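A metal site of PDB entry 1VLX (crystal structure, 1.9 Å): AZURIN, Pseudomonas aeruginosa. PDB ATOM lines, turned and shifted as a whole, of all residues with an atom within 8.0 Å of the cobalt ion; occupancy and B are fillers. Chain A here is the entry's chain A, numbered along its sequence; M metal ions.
The side-chain sulfur (SD) of Met 121 sits close to a ring nitrogen (ND1) of His 46 (3.5 Å).
A ring nitrogen (NE2) of His 46 sits at hydrogen-bond distance from the backbone carbonyl oxygen of Met 44, 3.4 Å away.
NE2 of His 46 lies within hydrogen-bond range of O of Asn 10.
O of His 46 sits at hydrogen-bond distance from N of Ile 87 (2.8 Å).
The backbone NH of Cys 112 sits at hydrogen-bond distance from the backbone carbonyl oxygen of Met 121 (3.2 Å).
The side-chain sulfur (SG) of Cys 112 lies close to the backbone NH (N) of Phe 114 (3.7 Å).
The side-chain sulfur of Cys 112 lies close to the backbone NH of Asn 47 (3.7 Å).
The side-chain sulfur of Met 13 sits close to a ring nitrogen (NE2) of His 117 (3.5 Å).
Merely in contact with the cobalt ion: Phe 114 (3.8 Å) and Met 121 (3.6 Å).
The cobalt ion is bound by O of Gly 45 (2.1 Å), ND1 of His 46 (2.3 Å), SG of Cys 112 (2.4 Å) and ND1 of His 117 (2.4 Å).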
ATOM      1  N   GLY A   9       9.573  30.351  15.887  1.00  0.00           N
ATOM      2  CA  GLY A   9      10.647  29.549  15.335  1.00  0.00           C
ATOM      3  C   GLY A   9      10.477  29.770  13.850  1.00  0.00           C
ATOM      4  O   GLY A   9       9.362  29.655  13.334  1.00  0.00           O
ATOM      5  N   ASN A  10      11.538  30.158  13.156  1.00  0.00           N
ATOM      6  CA  ASN A  10      11.442  30.464  11.710  1.00  0.00           C
ATOM      7  C   ASN A  10      12.102  29.467  10.752  1.00  0.00           C
ATOM      8  O   ASN A  10      12.543  28.404  11.145  1.00  0.00           O
ATOM      9  CB  ASN A  10      11.978  31.870  11.430  1.00  0.00           C
ATOM     10  CG  ASN A  10      13.458  31.992  11.714  1.00  0.00           C
ATOM     11  OD1 ASN A  10      14.179  31.002  11.677  1.00  0.00           O
ATOM     12  ND2 ASN A  10      13.934  33.211  11.984  1.00  0.00           N
ATOM     13  N   MET A  13      16.045  28.477  11.177  1.00  0.00           N
ATOM     14  CA  MET A  13      16.414  27.763  12.383  1.00  0.00           C
ATOM     15  C   MET A  13      16.738  28.677  13.553  1.00  0.00           C
ATOM     16  O   MET A  13      17.741  28.473  14.212  1.00  0.00           O
ATOM     17  CB  MET A  13      17.630  26.869  12.141  1.00  0.00           C
ATOM     18  CG  MET A  13      17.446  25.772  11.130  1.00  0.00           C
ATOM     19  SD  MET A  13      18.676  24.518  11.415  1.00  0.00           S
ATOM     20  CE  MET A  13      20.210  25.464  11.180  1.00  0.00           C
ATOM     21  N   GLN A  14      15.910  29.667  13.820  1.00  0.00           N
ATOM     22  CA  GLN A  14      16.177  30.613  14.906  1.00  0.00           C
ATOM     23  C   GLN A  14      14.934  30.865  15.734  1.00  0.00           C
ATOM     24  O   GLN A  14      13.817  30.795  15.221  1.00  0.00           O
ATOM     25  CB  GLN A  14      16.639  31.954  14.303  1.00  0.00           C
ATOM     26  CG  GLN A  14      17.879  31.925  13.397  1.00  0.00           C
ATOM     27  CD  GLN A  14      18.223  33.284  12.775  1.00  0.00           C
ATOM     28  OE1 GLN A  14      17.351  33.977  12.243  1.00  0.00           O
ATOM     29  NE2 GLN A  14      19.480  33.659  12.834  1.00  0.00           N
ATOM     30  N   PHE A  15      15.107  31.097  17.034  1.00  0.00           N
ATOM     31  CA  PHE A  15      13.997  31.407  17.907  1.00  0.00           C
ATOM     32  C   PHE A  15      14.124  32.919  18.004  1.00  0.00           C
ATOM     33  O   PHE A  15      15.225  33.452  17.910  1.00  0.00           O
ATOM     34  CB  PHE A  15      14.199  30.833  19.349  1.00  0.00           C
ATOM     35  CG  PHE A  15      13.732  29.396  19.538  1.00  0.00           C
ATOM     36  CD1 PHE A  15      12.508  28.948  19.098  1.00  0.00           C
ATOM     37  CD2 PHE A  15      14.526  28.517  20.264  1.00  0.00           C
ATOM     38  CE1 PHE A  15      12.055  27.620  19.391  1.00  0.00           C
ATOM     39  CE2 PHE A  15      14.091  27.212  20.550  1.00  0.00           C
ATOM     40  CZ  PHE A  15      12.862  26.767  20.123  1.00  0.00           C
ATOM     41  N   HIS A  35       5.237  29.184  14.261  1.00  0.00           N
ATOM     42  CA  HIS A  35       6.284  28.974  13.262  1.00  0.00           C
ATOM     43  C   HIS A  35       6.054  29.793  11.975  1.00  0.00           C
ATOM     44  O   HIS A  35       5.483  29.286  11.001  1.00  0.00           O
ATOM     45  CB  HIS A  35       6.272  27.483  12.924  1.00  0.00           C
ATOM     46  CG  HIS A  35       7.392  27.023  12.045  1.00  0.00           C
ATOM     47  ND1 HIS A  35       7.982  27.806  11.066  1.00  0.00           N
ATOM     48  CD2 HIS A  35       7.952  25.801  11.925  1.00  0.00           C
ATOM     49  CE1 HIS A  35       8.832  27.079  10.372  1.00  0.00           C
ATOM     50  NE2 HIS A  35       8.838  25.854  10.871  1.00  0.00           N
ATOM     51  N   LYS A  41       6.874  20.401   8.267  1.00  0.00           N
ATOM     52  CA  LYS A  41       7.405  19.727   9.440  1.00  0.00           C
ATOM     53  C   LYS A  41       8.598  18.798   9.268  1.00  0.00           C
ATOM     54  O   LYS A  41       9.466  18.804  10.104  1.00  0.00           O
ATOM     55  CB  LYS A  41       6.276  18.986  10.170  1.00  0.00           C
ATOM     56  CG  LYS A  41       6.655  18.531  11.535  1.00  0.00           C
ATOM     57  CD  LYS A  41       5.612  17.562  12.082  1.00  0.00           C
ATOM     58  CE  LYS A  41       4.231  18.181  12.156  1.00  0.00           C
ATOM     59  NZ  LYS A  41       3.256  17.184  12.719  1.00  0.00           N
ATOM     60  N   VAL A  43      10.972  19.085   7.293  1.00  0.00           N
ATOM     61  CA  VAL A  43      12.133  19.862   6.908  1.00  0.00           C
ATOM     62  C   VAL A  43      12.579  20.914   7.921  1.00  0.00           C
ATOM     63  O   VAL A  43      13.779  21.047   8.226  1.00  0.00           O
ATOM     64  CB  VAL A  43      11.880  20.546   5.536  1.00  0.00           C
ATOM     65  CG1 VAL A  43      12.980  21.453   5.197  1.00  0.00           C
ATOM     66  CG2 VAL A  43      11.784  19.525   4.456  1.00  0.00           C
ATOM     67  N   MET A  44      11.623  21.717   8.408  1.00  0.00           N
ATOM     68  CA  MET A  44      11.943  22.806   9.341  1.00  0.00           C
ATOM     69  C   MET A  44      11.079  22.686  10.583  1.00  0.00           C
ATOM     70  O   MET A  44      10.530  23.688  11.055  1.00  0.00           O
ATOM     71  CB  MET A  44      11.758  24.170   8.639  1.00  0.00           C
ATOM     72  CG  MET A  44      12.500  25.403   9.218  1.00  0.00           C
ATOM     73  SD  MET A  44      14.155  25.117   9.838  1.00  0.00           S
ATOM     74  CE  MET A  44      15.243  25.083   8.362  1.00  0.00           C
ATOM     75  N   GLY A  45      10.954  21.463  11.085  1.00  0.00           N
ATOM     76  CA  GLY A  45      10.190  21.209  12.297  1.00  0.00           C
ATOM     77  C   GLY A  45      10.656  21.910  13.573  1.00  0.00           C
ATOM     78  O   GLY A  45      11.877  22.058  13.866  1.00  0.00           O
ATOM     79  N   HIS A  46       9.720  22.427  14.339  1.00  0.00           N
ATOM     80  CA  HIS A  46      10.041  23.122  15.599  1.00  0.00           C
ATOM     81  C   HIS A  46       9.173  22.728  16.781  1.00  0.00           C
ATOM     82  O   HIS A  46       7.944  22.651  16.622  1.00  0.00           O
ATOM     83  CB  HIS A  46       9.948  24.666  15.410  1.00  0.00           C
ATOM     84  CG  HIS A  46      10.909  25.240  14.399  1.00  0.00           C
ATOM     85  ND1 HIS A  46      12.204  24.806  14.270  1.00  0.00           N
ATOM     86  CD2 HIS A  46      10.743  26.200  13.468  1.00  0.00           C
ATOM     87  CE1 HIS A  46      12.798  25.461  13.286  1.00  0.00           C
ATOM     88  NE2 HIS A  46      11.930  26.312  12.779  1.00  0.00           N
ATOM     89  N   ASN A  47       9.757  22.279  17.804  1.00  0.00           N
ATOM     90  CA  ASN A  47       9.060  22.107  19.076  1.00  0.00           C
ATOM     91  C   ASN A  47       9.820  22.836  20.155  1.00  0.00           C
ATOM     92  O   ASN A  47      11.011  23.130  20.014  1.00  0.00           O
ATOM     93  CB  ASN A  47       8.923  20.605  19.408  1.00  0.00           C
ATOM     94  CG  ASN A  47      10.256  19.875  19.613  1.00  0.00           C
ATOM     95  OD1 ASN A  47      11.304  20.517  19.660  1.00  0.00           O
ATOM     96  ND2 ASN A  47      10.283  18.564  19.745  1.00  0.00           N
ATOM     97  N   TRP A  48       8.875  23.096  21.166  1.00  0.00           N
ATOM     98  CA  TRP A  48       9.664  23.760  22.210  1.00  0.00           C
ATOM     99  C   TRP A  48       9.711  22.887  23.470  1.00  0.00           C
ATOM    100  O   TRP A  48       8.676  22.389  23.938  1.00  0.00           O
ATOM    101  CB  TRP A  48       9.046  25.106  22.573  1.00  0.00           C
ATOM    102  CG  TRP A  48       9.980  25.909  23.453  1.00  0.00           C
ATOM    103  CD1 TRP A  48      10.915  26.777  23.052  1.00  0.00           C
ATOM    104  CD2 TRP A  48       9.982  25.870  24.868  1.00  0.00           C
ATOM    105  NE1 TRP A  48      11.605  27.203  24.232  1.00  0.00           N
ATOM    106  CE2 TRP A  48      11.067  26.623  25.283  1.00  0.00           C
ATOM    107  CE3 TRP A  48       9.203  25.212  25.822  1.00  0.00           C
ATOM    108  CZ2 TRP A  48      11.496  26.674  26.607  1.00  0.00           C
ATOM    109  CZ3 TRP A  48       9.603  25.315  27.162  1.00  0.00           C
ATOM    110  CH2 TRP A  48      10.708  26.000  27.538  1.00  0.00           C
ATOM    111  N   LEU A  86       5.618  18.923  17.634  1.00  0.00           N
ATOM    112  CA  LEU A  86       6.586  19.438  16.648  1.00  0.00           C
ATOM    113  C   LEU A  86       5.658  20.031  15.598  1.00  0.00           C
ATOM    114  O   LEU A  86       4.695  19.362  15.171  1.00  0.00           O
ATOM    115  CB  LEU A  86       7.372  18.308  16.018  1.00  0.00           C
ATOM    116  CG  LEU A  86       8.590  18.680  15.185  1.00  0.00           C
ATOM    117  CD1 LEU A  86       9.803  19.123  16.104  1.00  0.00           C
ATOM    118  CD2 LEU A  86       9.027  17.411  14.439  1.00  0.00           C
ATOM    119  N   ILE A  87       5.858  21.313  15.320  1.00  0.00           N
ATOM    120  CA  ILE A  87       5.043  22.019  14.332  1.00  0.00           C
ATOM    121  C   ILE A  87       5.817  22.558  13.118  1.00  0.00           C
ATOM    122  O   ILE A  87       7.032  22.824  13.164  1.00  0.00           O
ATOM    123  CB  ILE A  87       4.310  23.200  14.955  1.00  0.00           C
ATOM    124  CG1 ILE A  87       5.315  24.208  15.510  1.00  0.00           C
ATOM    125  CG2 ILE A  87       3.334  22.733  16.027  1.00  0.00           C
ATOM    126  CD1 ILE A  87       4.700  25.523  15.889  1.00  0.00           C
ATOM    127  N   PHE A 111      14.654  24.369  24.120  1.00  0.00           N
ATOM    128  CA  PHE A 111      15.315  23.973  22.925  1.00  0.00           C
ATOM    129  C   PHE A 111      14.432  23.144  21.977  1.00  0.00           C
ATOM    130  O   PHE A 111      13.422  22.575  22.394  1.00  0.00           O
ATOM    131  CB  PHE A 111      16.624  23.230  23.319  1.00  0.00           C
ATOM    132  CG  PHE A 111      16.386  22.007  24.204  1.00  0.00           C
ATOM    133  CD1 PHE A 111      16.090  20.790  23.645  1.00  0.00           C
ATOM    134  CD2 PHE A 111      16.460  22.099  25.592  1.00  0.00           C
ATOM    135  CE1 PHE A 111      15.880  19.673  24.423  1.00  0.00           C
ATOM    136  CE2 PHE A 111      16.240  20.966  26.417  1.00  0.00           C
ATOM    137  CZ  PHE A 111      15.950  19.755  25.828  1.00  0.00           C
ATOM    138  N   CYS A 112      14.897  22.973  20.768  1.00  0.00           N
ATOM    139  CA  CYS A 112      14.242  22.231  19.709  1.00  0.00           C
ATOM    140  C   CYS A 112      14.954  20.884  19.561  1.00  0.00           C
ATOM    141  O   CYS A 112      16.215  20.831  19.422  1.00  0.00           O
ATOM    142  CB  CYS A 112      14.370  23.004  18.393  1.00  0.00           C
ATOM    143  SG  CYS A 112      13.390  22.255  17.102  1.00  0.00           S
ATOM    144  N   THR A 113      14.193  19.800  19.529  1.00  0.00           N
ATOM    145  CA  THR A 113      14.812  18.493  19.367  1.00  0.00           C
ATOM    146  C   THR A 113      14.873  17.923  17.959  1.00  0.00           C
ATOM    147  O   THR A 113      15.239  16.759  17.821  1.00  0.00           O
ATOM    148  CB  THR A 113      14.174  17.415  20.266  1.00  0.00           C
ATOM    149  OG1 THR A 113      12.753  17.447  20.108  1.00  0.00           O
ATOM    150  CG2 THR A 113      14.574  17.642  21.739  1.00  0.00           C
ATOM    151  N   PHE A 114      14.350  18.644  16.956  1.00  0.00           N
ATOM    152  CA  PHE A 114      14.419  18.192  15.562  1.00  0.00           C
ATOM    153  C   PHE A 114      15.913  18.020  15.199  1.00  0.00           C
ATOM    154  O   PHE A 114      16.759  18.867  15.538  1.00  0.00           O
ATOM    155  CB  PHE A 114      13.742  19.235  14.671  1.00  0.00           C
ATOM    156  CG  PHE A 114      13.576  18.808  13.243  1.00  0.00           C
ATOM    157  CD1 PHE A 114      14.634  18.929  12.339  1.00  0.00           C
ATOM    158  CD2 PHE A 114      12.361  18.274  12.811  1.00  0.00           C
ATOM    159  CE1 PHE A 114      14.482  18.554  11.028  1.00  0.00           C
ATOM    160  CE2 PHE A 114      12.199  17.892  11.505  1.00  0.00           C
ATOM    161  CZ  PHE A 114      13.255  18.027  10.598  1.00  0.00           C
ATOM    162  N   PRO A 115      16.263  16.897  14.540  1.00  0.00           N
ATOM    163  CA  PRO A 115      17.663  16.626  14.149  1.00  0.00           C
ATOM    164  C   PRO A 115      18.541  17.837  13.675  1.00  0.00           C
ATOM    165  O   PRO A 115      18.230  18.522  12.685  1.00  0.00           O
ATOM    166  CB  PRO A 115      17.493  15.478  13.133  1.00  0.00           C
ATOM    167  CG  PRO A 115      16.303  14.700  13.678  1.00  0.00           C
ATOM    168  CD  PRO A 115      15.338  15.855  14.000  1.00  0.00           C
ATOM    169  N   GLY A 116      19.538  18.152  14.495  1.00  0.00           N
ATOM    170  CA  GLY A 116      20.443  19.248  14.168  1.00  0.00           C
ATOM    171  C   GLY A 116      20.029  20.683  14.464  1.00  0.00           C
ATOM    172  O   GLY A 116      20.806  21.613  14.205  1.00  0.00           O
ATOM    173  N   HIS A 117      18.844  20.890  15.014  1.00  0.00           N
ATOM    174  CA  HIS A 117      18.376  22.236  15.318  1.00  0.00           C
ATOM    175  C   HIS A 117      18.758  22.817  16.684  1.00  0.00           C
ATOM    176  O   HIS A 117      18.806  24.042  16.796  1.00  0.00           O
ATOM    177  CB  HIS A 117      16.875  22.316  15.165  1.00  0.00           C
ATOM    178  CG  HIS A 117      16.431  22.184  13.753  1.00  0.00           C
ATOM    179  ND1 HIS A 117      15.119  22.296  13.354  1.00  0.00           N
ATOM    180  CD2 HIS A 117      17.150  21.970  12.629  1.00  0.00           C
ATOM    181  CE1 HIS A 117      15.048  22.189  12.041  1.00  0.00           C
ATOM    182  NE2 HIS A 117      16.268  21.986  11.580  1.00  0.00           N
ATOM    183  N   SER A 118      19.036  21.969  17.678  1.00  0.00           N
ATOM    184  CA  SER A 118      19.356  22.425  19.042  1.00  0.00           C
ATOM    185  C   SER A 118      20.667  23.164  19.236  1.00  0.00           C
ATOM    186  O   SER A 118      20.855  23.855  20.237  1.00  0.00           O
ATOM    187  CB  SER A 118      19.231  21.263  20.065  1.00  0.00           C
ATOM    188  OG  SER A 118      20.022  20.121  19.735  1.00  0.00           O
ATOM    189  N   MET A 121      19.100  26.282  18.102  1.00  0.00           N
ATOM    190  CA  MET A 121      17.834  26.688  18.737  1.00  0.00           C
ATOM    191  C   MET A 121      17.795  26.201  20.182  1.00  0.00           C
ATOM    192  O   MET A 121      17.220  25.155  20.485  1.00  0.00           O
ATOM    193  CB  MET A 121      16.658  26.100  17.961  1.00  0.00           C
ATOM    194  CG  MET A 121      16.560  26.656  16.548  1.00  0.00           C
ATOM    195  SD  MET A 121      15.098  26.150  15.681  1.00  0.00           S
ATOM    196  CE  MET A 121      13.734  27.222  16.102  1.00  0.00           C
HETATM  197 CO    CO M   1      13.474  23.053  14.885  1.00  0.00          CO
